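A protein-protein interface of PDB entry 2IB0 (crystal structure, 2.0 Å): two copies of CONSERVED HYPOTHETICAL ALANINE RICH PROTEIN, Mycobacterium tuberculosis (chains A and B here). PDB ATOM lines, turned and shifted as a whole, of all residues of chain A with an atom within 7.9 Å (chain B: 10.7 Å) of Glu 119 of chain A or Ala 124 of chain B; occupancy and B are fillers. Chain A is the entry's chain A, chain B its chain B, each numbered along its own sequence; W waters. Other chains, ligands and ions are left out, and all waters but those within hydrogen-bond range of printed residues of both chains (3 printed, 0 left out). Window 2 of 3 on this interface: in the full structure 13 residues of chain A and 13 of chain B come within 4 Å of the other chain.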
ATOM      1  N   GLU A  18      -0.913  -0.014   4.295  1.00  0.00           N
ATOM      2  CA  GLU A  18       0.499  -0.427   4.291  1.00  0.00           C
ATOM      3  C   GLU A  18       1.279   0.049   3.064  1.00  0.00           C
ATOM      4  O   GLU A  18       2.462   0.410   3.159  1.00  0.00           O
ATOM      5  CB  GLU A  18       0.607  -1.972   4.399  1.00  0.00           C
ATOM      6  CG  GLU A  18      -0.019  -2.586   5.652  1.00  0.00           C
ATOM      7  CD  GLU A  18       0.683  -2.136   6.918  1.00  0.00           C
ATOM      8  OE1 GLU A  18       1.781  -1.535   6.839  1.00  0.00           O
ATOM      9  OE2 GLU A  18       0.148  -2.354   8.014  1.00  0.00           O
ATOM     10  N   ALA A  21       1.751   3.732   3.189  1.00  0.00           N
ATOM     11  CA  ALA A  21       2.946   4.164   3.929  1.00  0.00           C
ATOM     12  C   ALA A  21       4.247   3.901   3.133  1.00  0.00           C
ATOM     13  O   ALA A  21       5.176   4.711   3.166  1.00  0.00           O
ATOM     14  CB  ALA A  21       3.017   3.476   5.311  1.00  0.00           C
ATOM     15  N   ASP A  22       4.284   2.766   2.419  1.00  0.00           N
ATOM     16  CA  ASP A  22       5.393   2.386   1.529  1.00  0.00           C
ATOM     17  C   ASP A  22       5.616   3.471   0.451  1.00  0.00           C
ATOM     18  O   ASP A  22       6.723   4.015   0.335  1.00  0.00           O
ATOM     19  CB  ASP A  22       5.094   0.999   0.900  1.00  0.00           C
ATOM     20  CG  ASP A  22       6.316   0.333   0.281  1.00  0.00           C
ATOM     21  OD1 ASP A  22       7.406   0.978   0.158  1.00  0.00           O
ATOM     22  OD2 ASP A  22       6.190  -0.888  -0.061  1.00  0.00           O
ATOM     23  N   ALA A  25       6.743   6.740   1.998  1.00  0.00           N
ATOM     24  CA  ALA A  25       8.128   6.761   2.391  1.00  0.00           C
ATOM     25  C   ALA A  25       9.037   6.929   1.170  1.00  0.00           C
ATOM     26  O   ALA A  25      10.049   7.572   1.254  1.00  0.00           O
ATOM     27  CB  ALA A  25       8.510   5.468   3.206  1.00  0.00           C
ATOM     28  N   THR A 112      18.188   9.091   7.251  1.00  0.00           N
ATOM     29  CA  THR A 112      16.875   9.166   7.912  1.00  0.00           C
ATOM     30  C   THR A 112      15.715   8.822   6.999  1.00  0.00           C
ATOM     31  O   THR A 112      14.780   8.138   7.434  1.00  0.00           O
ATOM     32  CB  THR A 112      16.636  10.551   8.512  1.00  0.00           C
ATOM     33  OG1 THR A 112      17.649  10.797   9.475  1.00  0.00           O
ATOM     34  CG2 THR A 112      15.261  10.640   9.212  1.00  0.00           C
ATOM     35  N   ALA A 113      15.755   9.317   5.759  1.00  0.00           N
ATOM     36  CA  ALA A 113      14.672   9.076   4.790  1.00  0.00           C
ATOM     37  C   ALA A 113      14.713   7.616   4.286  1.00  0.00           C
ATOM     38  O   ALA A 113      13.694   6.972   4.166  1.00  0.00           O
ATOM     39  CB  ALA A 113      14.749  10.036   3.638  1.00  0.00           C
ATOM     40  N   TRP A 114      15.903   7.105   4.026  1.00  0.00           N
ATOM     41  CA  TRP A 114      16.064   5.696   3.676  1.00  0.00           C
ATOM     42  C   TRP A 114      15.742   4.695   4.774  1.00  0.00           C
ATOM     43  O   TRP A 114      15.179   3.638   4.486  1.00  0.00           O
ATOM     44  CB  TRP A 114      17.420   5.432   3.013  1.00  0.00           C
ATOM     45  CG  TRP A 114      17.407   6.106   1.649  1.00  0.00           C
ATOM     46  CD1 TRP A 114      18.103   7.225   1.278  1.00  0.00           C
ATOM     47  CD2 TRP A 114      16.615   5.729   0.521  1.00  0.00           C
ATOM     48  NE1 TRP A 114      17.809   7.561  -0.022  1.00  0.00           N
ATOM     49  CE2 TRP A 114      16.896   6.658  -0.513  1.00  0.00           C
ATOM     50  CE3 TRP A 114      15.696   4.686   0.277  1.00  0.00           C
ATOM     51  CZ2 TRP A 114      16.318   6.576  -1.769  1.00  0.00           C
ATOM     52  CZ3 TRP A 114      15.088   4.615  -0.984  1.00  0.00           C
ATOM     53  CH2 TRP A 114      15.400   5.559  -1.990  1.00  0.00           C
ATOM     54  N   ARG A 115      16.068   5.007   6.026  1.00  0.00           N
ATOM     55  CA  ARG A 115      15.628   4.138   7.127  1.00  0.00           C
ATOM     56  C   ARG A 115      14.110   4.044   7.155  1.00  0.00           C
ATOM     57  O   ARG A 115      13.577   3.002   7.475  1.00  0.00           O
ATOM     58  CB  ARG A 115      16.164   4.631   8.464  1.00  0.00           C
ATOM     59  CG  ARG A 115      15.831   3.735   9.606  1.00  0.00           C
ATOM     60  CD  ARG A 115      16.506   4.206  10.900  1.00  0.00           C
ATOM     61  NE  ARG A 115      17.928   4.465  10.695  1.00  0.00           N
ATOM     62  CZ  ARG A 115      18.501   5.665  10.677  1.00  0.00           C
ATOM     63  NH1 ARG A 115      17.780   6.782  10.864  1.00  0.00           N
ATOM     64  NH2 ARG A 115      19.816   5.745  10.475  1.00  0.00           N
ATOM     65  N   ALA A 116      13.406   5.131   6.823  1.00  0.00           N
ATOM     66  CA  ALA A 116      11.930   5.057   6.756  1.00  0.00           C
ATOM     67  C   ALA A 116      11.410   4.145   5.644  1.00  0.00           C
ATOM     68  O   ALA A 116      10.398   3.491   5.810  1.00  0.00           O
ATOM     69  CB  ALA A 116      11.330   6.449   6.614  1.00  0.00           C
ATOM     70  N   VAL A 117      12.067   4.155   4.480  1.00  0.00           N
ATOM     71  CA  VAL A 117      11.714   3.207   3.412  1.00  0.00           C
ATOM     72  C   VAL A 117      11.988   1.735   3.855  1.00  0.00           C
ATOM     73  O   VAL A 117      11.147   0.812   3.635  1.00  0.00           O
ATOM     74  CB  VAL A 117      12.426   3.588   2.062  1.00  0.00           C
ATOM     75  CG1 VAL A 117      12.073   2.587   0.966  1.00  0.00           C
ATOM     76  CG2 VAL A 117      12.027   5.078   1.566  1.00  0.00           C
ATOM     77  N   VAL A 118      13.148   1.490   4.483  1.00  0.00           N
ATOM     78  CA  VAL A 118      13.421   0.115   5.011  1.00  0.00           C
ATOM     79  C   VAL A 118      12.258  -0.325   5.882  1.00  0.00           C
ATOM     80  O   VAL A 118      11.788  -1.471   5.800  1.00  0.00           O
ATOM     81  CB  VAL A 118      14.752   0.002   5.880  1.00  0.00           C
ATOM     82  CG1 VAL A 118      14.887  -1.389   6.587  1.00  0.00           C
ATOM     83  CG2 VAL A 118      15.981   0.305   5.056  1.00  0.00           C
ATOM     84  N   GLU A 119      11.855   0.570   6.782  1.00  0.00           N
ATOM     85  CA  GLU A 119      10.828   0.282   7.759  1.00  0.00           C
ATOM     86  C   GLU A 119       9.436  -0.021   7.126  1.00  0.00           C
ATOM     87  O   GLU A 119       8.747  -0.940   7.547  1.00  0.00           O
ATOM     88  CB  GLU A 119      10.756   1.482   8.703  1.00  0.00           C
ATOM     89  CG  GLU A 119       9.715   1.299   9.795  1.00  0.00           C
ATOM     90  CD  GLU A 119       9.721   2.441  10.797  1.00  0.00           C
ATOM     91  OE1 GLU A 119      10.392   3.460  10.562  1.00  0.00           O
ATOM     92  OE2 GLU A 119       9.061   2.299  11.837  1.00  0.00           O
ATOM     93  N   HIS A 120       9.045   0.756   6.110  1.00  0.00           N
ATOM     94  CA  HIS A 120       7.702   0.635   5.503  1.00  0.00           C
ATOM     95  C   HIS A 120       7.661  -0.114   4.167  1.00  0.00           C
ATOM     96  O   HIS A 120       6.582  -0.303   3.624  1.00  0.00           O
ATOM     97  CB  HIS A 120       7.048   2.018   5.311  1.00  0.00           C
ATOM     98  CG  HIS A 120       6.887   2.795   6.589  1.00  0.00           C
ATOM     99  ND1 HIS A 120       6.035   2.392   7.597  1.00  0.00           N
ATOM    100  CD2 HIS A 120       7.470   3.927   7.026  1.00  0.00           C
ATOM    101  CE1 HIS A 120       6.112   3.233   8.607  1.00  0.00           C
ATOM    102  NE2 HIS A 120       6.967   4.181   8.284  1.00  0.00           N
ATOM    103  N   ALA A 121       8.808  -0.555   3.653  1.00  0.00           N
ATOM    104  CA  ALA A 121       8.820  -1.244   2.346  1.00  0.00           C
ATOM    105  C   ALA A 121       8.294  -2.635   2.518  1.00  0.00           C
ATOM    106  O   ALA A 121       8.824  -3.397   3.338  1.00  0.00           O
ATOM    107  CB  ALA A 121      10.200  -1.299   1.754  1.00  0.00           C
ATOM    108  N   GLU A 122       7.283  -2.982   1.719  1.00  0.00           N
ATOM    109  CA  GLU A 122       6.632  -4.330   1.811  1.00  0.00           C
ATOM    110  C   GLU A 122       7.447  -5.456   1.213  1.00  0.00           C
ATOM    111  O   GLU A 122       7.448  -6.601   1.743  1.00  0.00           O
ATOM    112  CB  GLU A 122       5.244  -4.293   1.208  1.00  0.00           C
ATOM    113  CG  GLU A 122       4.337  -3.234   1.832  1.00  0.00           C
ATOM    114  CD  GLU A 122       2.898  -3.556   1.665  1.00  0.00           C
ATOM    115  OE1 GLU A 122       2.322  -3.021   0.708  1.00  0.00           O
ATOM    116  OE2 GLU A 122       2.353  -4.374   2.462  1.00  0.00           O
ATOM    117  N   ARG A 127      13.189  -3.244   0.270  1.00  0.00           N
ATOM    118  CA  ARG A 127      13.964  -3.084   1.500  1.00  0.00           C
ATOM    119  C   ARG A 127      15.463  -3.241   1.298  1.00  0.00           C
ATOM    120  O   ARG A 127      16.241  -2.528   1.938  1.00  0.00           O
ATOM    121  CB  ARG A 127      13.547  -4.068   2.588  1.00  0.00           C
ATOM    122  CG  ARG A 127      12.161  -3.879   3.087  1.00  0.00           C
ATOM    123  CD  ARG A 127      11.998  -4.707   4.343  1.00  0.00           C
ATOM    124  NE  ARG A 127      12.246  -6.138   4.185  1.00  0.00           N
ATOM    125  CZ  ARG A 127      11.357  -7.004   3.702  1.00  0.00           C
ATOM    126  NH1 ARG A 127      10.155  -6.575   3.287  1.00  0.00           N
ATOM    127  NH2 ARG A 127      11.665  -8.302   3.633  1.00  0.00           N
ATOM    128  N   ALA A 130      16.612   0.033  -0.294  1.00  0.00           N
ATOM    129  CA  ALA A 130      16.557   1.131   0.653  1.00  0.00           C
ATOM    130  C   ALA A 130      17.732   0.988   1.640  1.00  0.00           C
ATOM    131  O   ALA A 130      18.344   1.970   1.987  1.00  0.00           O
ATOM    132  CB  ALA A 130      15.220   1.145   1.399  1.00  0.00           C
ATOM    133  N   SER A 131      18.025  -0.246   2.087  1.00  0.00           N
ATOM    134  CA  SER A 131      19.131  -0.447   2.978  1.00  0.00           C
ATOM    135  C   SER A 131      20.477  -0.168   2.334  1.00  0.00           C
ATOM    136  O   SER A 131      21.366   0.336   3.007  1.00  0.00           O
ATOM    137  CB  SER A 131      19.108  -1.817   3.666  1.00  0.00           C
ATOM    138  OG  SER A 131      19.693  -2.834   2.863  1.00  0.00           O
ATOM    139  N   LEU A 134      20.605   3.529   2.324  1.00  0.00           N
ATOM    140  CA  LEU A 134      20.843   3.989   3.673  1.00  0.00           C
ATOM    141  C   LEU A 134      22.352   3.870   4.037  1.00  0.00           C
ATOM    142  O   LEU A 134      22.965   4.795   4.595  1.00  0.00           O
ATOM    143  CB  LEU A 134      20.017   3.135   4.643  1.00  0.00           C
ATOM    144  CG  LEU A 134      19.699   3.521   6.096  1.00  0.00           C
ATOM    145  CD1 LEU A 134      19.308   2.309   6.839  1.00  0.00           C
ATOM    146  CD2 LEU A 134      20.798   4.189   6.829  1.00  0.00           C
ATOM    147  N   ASP B  22      13.389 -16.332   8.871  1.00  0.00           N
ATOM    148  CA  ASP B  22      13.710 -15.164   9.701  1.00  0.00           C
ATOM    149  C   ASP B  22      14.686 -15.586  10.788  1.00  0.00           C
ATOM    150  O   ASP B  22      15.742 -14.978  10.942  1.00  0.00           O
ATOM    151  CB  ASP B  22      12.421 -14.547  10.303  1.00  0.00           C
ATOM    152  CG  ASP B  22      12.642 -13.153  10.913  1.00  0.00           C
ATOM    153  OD1 ASP B  22      13.802 -12.706  11.160  1.00  0.00           O
ATOM    154  OD2 ASP B  22      11.636 -12.461  11.138  1.00  0.00           O
ATOM    155  N   MET B  72      16.832 -10.857  21.311  1.00  0.00           N
ATOM    156  CA  MET B  72      15.806 -10.953  20.246  1.00  0.00           C
ATOM    157  C   MET B  72      15.428 -12.421  20.001  1.00  0.00           C
ATOM    158  O   MET B  72      14.245 -12.751  19.880  1.00  0.00           O
ATOM    159  CB  MET B  72      16.260 -10.305  18.918  1.00  0.00           C
ATOM    160  CG  MET B  72      16.476  -8.820  18.952  1.00  0.00           C
ATOM    161  SD  MET B  72      17.550  -8.284  17.605  1.00  0.00           S
ATOM    162  CE  MET B  72      16.427  -8.459  16.203  1.00  0.00           C
ATOM    163  N   ARG B  76      11.880 -14.592  20.653  1.00  0.00           N
ATOM    164  CA  ARG B  76      11.366 -15.525  19.639  1.00  0.00           C
ATOM    165  C   ARG B  76      11.148 -16.975  20.161  1.00  0.00           C
ATOM    166  O   ARG B  76      10.476 -17.768  19.498  1.00  0.00           O
ATOM    167  CB  ARG B  76      12.281 -15.534  18.388  1.00  0.00           C
ATOM    168  CG  ARG B  76      12.308 -14.216  17.595  1.00  0.00           C
ATOM    169  CD  ARG B  76      13.118 -14.351  16.313  1.00  0.00           C
ATOM    170  NE  ARG B  76      13.170 -13.086  15.590  1.00  0.00           N
ATOM    171  CZ  ARG B  76      13.650 -12.949  14.369  1.00  0.00           C
ATOM    172  NH1 ARG B  76      14.116 -14.015  13.729  1.00  0.00           N
ATOM    173  NH2 ARG B  76      13.698 -11.740  13.795  1.00  0.00           N
ATOM    174  N   VAL B 117      19.230 -10.585   6.937  1.00  0.00           N
ATOM    175  CA  VAL B 117      18.242 -10.357   8.013  1.00  0.00           C
ATOM    176  C   VAL B 117      17.282  -9.253   7.604  1.00  0.00           C
ATOM    177  O   VAL B 117      16.042  -9.386   7.821  1.00  0.00           O
ATOM    178  CB  VAL B 117      18.924 -10.060   9.397  1.00  0.00           C
ATOM    179  CG1 VAL B 117      17.884  -9.811  10.499  1.00  0.00           C
ATOM    180  CG2 VAL B 117      19.806 -11.232   9.851  1.00  0.00           C
ATOM    181  N   VAL B 118      17.802  -8.180   6.958  1.00  0.00           N
ATOM    182  CA  VAL B 118      16.899  -7.190   6.390  1.00  0.00           C
ATOM    183  C   VAL B 118      15.910  -7.831   5.428  1.00  0.00           C
ATOM    184  O   VAL B 118      14.729  -7.525   5.496  1.00  0.00           O
ATOM    185  CB  VAL B 118      17.609  -5.998   5.639  1.00  0.00           C
ATOM    186  CG1 VAL B 118      16.562  -5.098   5.020  1.00  0.00           C
ATOM    187  CG2 VAL B 118      18.547  -5.232   6.591  1.00  0.00           C
ATOM    188  N   GLU B 119      16.381  -8.697   4.519  1.00  0.00           N
ATOM    189  CA  GLU B 119      15.449  -9.339   3.567  1.00  0.00           C
ATOM    190  C   GLU B 119      14.428 -10.219   4.237  1.00  0.00           C
ATOM    191  O   GLU B 119      13.313 -10.229   3.814  1.00  0.00           O
ATOM    192  CB  GLU B 119      16.115 -10.308   2.589  1.00  0.00           C
ATOM    193  CG  GLU B 119      17.335  -9.904   1.916  1.00  0.00           C
ATOM    194  CD  GLU B 119      17.716 -10.947   0.849  1.00  0.00           C
ATOM    195  OE1 GLU B 119      18.891 -11.217   0.708  1.00  0.00           O
ATOM    196  OE2 GLU B 119      16.815 -11.510   0.177  1.00  0.00           O
ATOM    197  N   HIS B 120      14.851 -11.044   5.193  1.00  0.00           N
ATOM    198  CA  HIS B 120      13.990 -12.093   5.762  1.00  0.00           C
ATOM    199  C   HIS B 120      13.292 -11.744   7.056  1.00  0.00           C
ATOM    200  O   HIS B 120      12.378 -12.448   7.448  1.00  0.00           O
ATOM    201  CB  HIS B 120      14.808 -13.379   5.970  1.00  0.00           C
ATOM    202  CG  HIS B 120      15.308 -13.953   4.693  1.00  0.00           C
ATOM    203  ND1 HIS B 120      14.459 -14.299   3.666  1.00  0.00           N
ATOM    204  CD2 HIS B 120      16.561 -14.192   4.245  1.00  0.00           C
ATOM    205  CE1 HIS B 120      15.169 -14.750   2.646  1.00  0.00           C
ATOM    206  NE2 HIS B 120      16.444 -14.696   2.974  1.00  0.00           N
ATOM    207  N   ALA B 121      13.681 -10.654   7.711  1.00  0.00           N
ATOM    208  CA  ALA B 121      13.011 -10.270   8.955  1.00  0.00           C
ATOM    209  C   ALA B 121      11.572  -9.975   8.641  1.00  0.00           C
ATOM    210  O   ALA B 121      11.290  -9.199   7.733  1.00  0.00           O
ATOM    211  CB  ALA B 121      13.638  -9.042   9.570  1.00  0.00           C
ATOM    212  N   GLU B 122      10.652 -10.552   9.401  1.00  0.00           N
ATOM    213  CA  GLU B 122       9.218 -10.215   9.180  1.00  0.00           C
ATOM    214  C   GLU B 122       8.792  -8.845   9.724  1.00  0.00           C
ATOM    215  O   GLU B 122       8.037  -8.116   9.051  1.00  0.00           O
ATOM    216  CB  GLU B 122       8.342 -11.311   9.720  1.00  0.00           C
ATOM    217  CG  GLU B 122       8.668 -12.682   9.127  1.00  0.00           C
ATOM    218  CD  GLU B 122       7.496 -13.623   9.222  1.00  0.00           C
ATOM    219  OE1 GLU B 122       7.518 -14.506  10.112  1.00  0.00           O
ATOM    220  OE2 GLU B 122       6.554 -13.469   8.400  1.00  0.00           O
ATOM    221  N   THR B 123       9.264  -8.470  10.914  1.00  0.00           N
ATOM    222  CA  THR B 123       8.862  -7.182  11.514  1.00  0.00           C
ATOM    223  C   THR B 123       9.764  -5.992  11.157  1.00  0.00           C
ATOM    224  O   THR B 123      10.987  -6.137  10.919  1.00  0.00           O
ATOM    225  CB  THR B 123       8.718  -7.264  13.048  1.00  0.00           C
ATOM    226  OG1 THR B 123      10.011  -7.166  13.670  1.00  0.00           O
ATOM    227  CG2 THR B 123       8.012  -8.576  13.477  1.00  0.00           C
ATOM    228  N   ALA B 124       9.138  -4.823  11.101  1.00  0.00           N
ATOM    229  CA  ALA B 124       9.805  -3.564  10.869  1.00  0.00           C
ATOM    230  C   ALA B 124      10.865  -3.282  11.924  1.00  0.00           C
ATOM    231  O   ALA B 124      11.925  -2.799  11.567  1.00  0.00           O
ATOM    232  CB  ALA B 124       8.788  -2.397  10.800  1.00  0.00           C
ATOM    233  N   ASP B 125      10.564  -3.552  13.205  1.00  0.00           N
ATOM    234  CA  ASP B 125      11.539  -3.353  14.305  1.00  0.00           C
ATOM    235  C   ASP B 125      12.845  -4.116  14.066  1.00  0.00           C
ATOM    236  O   ASP B 125      13.920  -3.551  14.178  1.00  0.00           O
ATOM    237  CB  ASP B 125      10.970  -3.747  15.679  1.00  0.00           C
ATOM    238  CG  ASP B 125      10.040  -2.699  16.264  1.00  0.00           C
ATOM    239  OD1 ASP B 125      10.216  -1.478  16.024  1.00  0.00           O
ATOM    240  OD2 ASP B 125       9.102  -3.110  16.983  1.00  0.00           O
ATOM    241  N   ASP B 126      12.731  -5.400  13.751  1.00  0.00           N
ATOM    242  CA  ASP B 126      13.865  -6.246  13.434  1.00  0.00           C
ATOM    243  C   ASP B 126      14.528  -5.915  12.084  1.00  0.00           C
ATOM    244  O   ASP B 126      15.736  -6.068  11.918  1.00  0.00           O
ATOM    245  CB  ASP B 126      13.447  -7.699  13.427  1.00  0.00           C
ATOM    246  CG  ASP B 126      13.059  -8.213  14.798  1.00  0.00           C
ATOM    247  OD1 ASP B 126      13.175  -7.468  15.787  1.00  0.00           O
ATOM    248  OD2 ASP B 126      12.627  -9.380  14.876  1.00  0.00           O
ATOM    249  N   ARG B 127      13.753  -5.457  11.111  1.00  0.00           N
ATOM    250  CA  ARG B 127      14.378  -5.026   9.867  1.00  0.00           C
ATOM    251  C   ARG B 127      15.212  -3.765  10.075  1.00  0.00           C
ATOM    252  O   ARG B 127      16.281  -3.612   9.501  1.00  0.00           O
ATOM    253  CB  ARG B 127      13.330  -4.793   8.794  1.00  0.00           C
ATOM    254  CG  ARG B 127      12.911  -6.103   8.219  1.00  0.00           C
ATOM    255  CD  ARG B 127      11.973  -5.927   7.082  1.00  0.00           C
ATOM    256  NE  ARG B 127      11.097  -4.764   7.189  1.00  0.00           N
ATOM    257  CZ  ARG B 127       9.817  -4.833   7.523  1.00  0.00           C
ATOM    258  NH1 ARG B 127       9.288  -6.018   7.808  1.00  0.00           N
ATOM    259  NH2 ARG B 127       9.069  -3.715   7.553  1.00  0.00           N
ATOM    260  N   VAL B 128      14.712  -2.866  10.911  1.00  0.00           N
ATOM    261  CA  VAL B 128      15.420  -1.634  11.159  1.00  0.00           C
ATOM    262  C   VAL B 128      16.677  -1.912  11.987  1.00  0.00           C
ATOM    263  O   VAL B 128      17.717  -1.332  11.737  1.00  0.00           O
ATOM    264  CB  VAL B 128      14.527  -0.575  11.790  1.00  0.00           C
ATOM    265  CG1 VAL B 128      15.359   0.577  12.320  1.00  0.00           C
ATOM    266  CG2 VAL B 128      13.436  -0.096  10.762  1.00  0.00           C
ATOM    267  N   PHE B 129      16.582  -2.848  12.931  1.00  0.00           N
ATOM    268  CA  PHE B 129      17.741  -3.277  13.688  1.00  0.00           C
ATOM    269  C   PHE B 129      18.808  -3.826  12.763  1.00  0.00           C
ATOM    270  O   PHE B 129      20.006  -3.514  12.914  1.00  0.00           O
ATOM    271  CB  PHE B 129      17.356  -4.358  14.711  1.00  0.00           C
ATOM    272  CG  PHE B 129      18.522  -4.838  15.557  1.00  0.00           C
ATOM    273  CD1 PHE B 129      18.832  -4.215  16.759  1.00  0.00           C
ATOM    274  CD2 PHE B 129      19.324  -5.905  15.134  1.00  0.00           C
ATOM    275  CE1 PHE B 129      19.892  -4.681  17.531  1.00  0.00           C
ATOM    276  CE2 PHE B 129      20.387  -6.330  15.887  1.00  0.00           C
ATOM    277  CZ  PHE B 129      20.673  -5.720  17.090  1.00  0.00           C
ATOM    278  N   ALA B 130      18.400  -4.721  11.871  1.00  0.00           N
ATOM    279  CA  ALA B 130      19.332  -5.325  10.939  1.00  0.00           C
ATOM    280  C   ALA B 130      19.975  -4.278   9.995  1.00  0.00           C
ATOM    281  O   ALA B 130      21.175  -4.358   9.727  1.00  0.00           O
ATOM    282  CB  ALA B 130      18.647  -6.402  10.171  1.00  0.00           C
ATOM    283  N   SER B 131      19.188  -3.308   9.514  1.00  0.00           N
ATOM    284  CA  SER B 131      19.713  -2.177   8.709  1.00  0.00           C
ATOM    285  C   SER B 131      20.754  -1.363   9.440  1.00  0.00           C
ATOM    286  O   SER B 131      21.735  -0.983   8.852  1.00  0.00           O
ATOM    287  CB  SER B 131      18.599  -1.269   8.140  1.00  0.00           C
ATOM    288  OG  SER B 131      18.224  -0.190   9.009  1.00  0.00           O
ATOM    289  N   THR B 132      20.528  -1.080  10.717  1.00  0.00           N
ATOM    290  CA  THR B 132      21.537  -0.429  11.545  1.00  0.00           C
ATOM    291  C   THR B 132      22.838  -1.222  11.637  1.00  0.00           C
ATOM    292  O   THR B 132      23.914  -0.662  11.502  1.00  0.00           O
ATOM    293  CB  THR B 132      20.972  -0.142  12.942  1.00  0.00           C
ATOM    294  OG1 THR B 132      19.878   0.734  12.783  1.00  0.00           O
ATOM    295  CG2 THR B 132      21.993   0.560  13.839  1.00  0.00           C
HETATM  296  O   HOH W   1      19.131   1.900  10.547  1.00  0.00           O
HETATM  297  O   HOH W   2      21.046  -0.617   5.831  1.00  0.00           O
HETATM  298  O   HOH W   3       6.111  -2.930   5.879  1.00  0.00           O
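Val 118 of chain A touches Arg 127 of chain B, and with the chains exchanged Arg 127 of chain A touches Val 118 of chain B.
Glu 119 of chain A touches Arg 127 of chain B, and with the chains exchanged Arg 127 of chain A touches Glu 119 of chain B.
Arg 127 of chain B touches its own counterpart, Arg 127 of chain A.
Positions printed for both chains: 22, 117, 118, 119, 120, 121, 122, 127, 130 and 131.
Of the 8 pairs that touch across the chains among the printed residues, 5 have their exchanged pair printed and touching as well.
The guanidinium group (NH2) of Arg 127 of chain B sits at hydrogen-bond distance from the backbone carbonyl oxygen (O) of Glu 119 of chain A (2.8 Å).
The guanidinium group of Arg 127 of chain A sits at hydrogen-bond distance from the backbone carbonyl oxygen of Val 118 of chain B.
The backbone carbonyl oxygen of Glu 119 of chain B lies within hydrogen-bond range of the guanidinium group of Arg 127 of chain A.
The guanidinium group of Arg 127 of chain B sits close to the guanidinium group of Arg 127 of chain A (3.5 Å).
Ala 113 of chain A touches none of the printed residues of chain B.
No residue of chain B comes within 4 Å of Ala 116 of chain A.
Val 118 of chain A touches just one residue of chain B: Arg 127.
No residue of chain B comes within 4 Å of Ala 121 of chain A.
Of the printed residues of chain B, Leu 134 of chain A touches Ser 131.
Of the printed residues of chain A, Glu 119 of chain B touches Arg 127 (2.5 Å).
Ala 124 of chain B touches just one residue of chain A: Glu 119.
Of the printed residues of chain A, Arg 127 of chain B touches Val 118 (3.6 Å), Glu 119 (2.8 Å) and Arg 127 (2.9 Å).
Of the printed residues of chain A, Ser 131 of chain B touches Leu 134.
The nearest residue of chain B that does not touch Glu 119 of chain A is Asp 125 of chain B (5.8 Å).
The nearest printed residue of chain B that does not touch Leu 134 of chain A is Thr 132 of chain B (5.3 Å).
The backbone carbonyl oxygen (O) of Val 128 of chain B is in hydrogen-bond range of the side-chain hydroxyl (OG1) of Thr 132 of chain B (3.2 Å).
NH1 of Arg 127 of chain A is in hydrogen-bond range of O of Glu 122 of chain A.
The backbone carbonyl oxygen (O) of Val 128 of chain B sits at hydrogen-bond distance from the side-chain hydroxyl (OG) of Ser 131 of chain B.
NH1 of Arg 127 of chain A sits close to O of Ala 121 of chain A, at 3.4 Å.
The guanidinium group (NH1) of Arg 127 of chain B lies within hydrogen-bond range of the backbone carbonyl oxygen (O) of Glu 122 of chain B (2.7 Å).
Water W1 lies within hydrogen-bond range of OG1 of Thr 132 of chain B, OG of Ser 131 of chain B and NE of Arg 115 of chain A.
Water W2 lies within hydrogen-bond range of the backbone carbonyl oxygen (O) of Ser 131 of chain A (3.0 Å) and the backbone carbonyl oxygen (O) of Ser 131 of chain B (3.1 Å).
Water W3 lies within hydrogen-bond range of the guanidinium group (NH2) of Arg 127 of chain B (3.5 Å) and the backbone carbonyl oxygen (O) of His 120 of chain A (3.5 Å).
Hydrophobic or aromatic side chains of chain A that line the printed part of chain B: Val 118 and Leu 134.
Of the 19 printed residues of chain B, 6 touch a printed residue of chain A.
Among the printed residues, no Asp or Glu carboxylate lies within 4 Å of a Lys or Arg side-chain nitrogen of the other chain.
Among the printed residues, merely in contact across the chains: Leu 134 of chain A with Ser 131 of chain B (3.5 Å), Glu 119 of chain A with Ala 124 of chain B (3.6 Å), Val 118 of chain A with Arg 127 of chain B (3.6 Å) and Glu 119 of chain A with Val 128 of chain B (3.7 Å).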
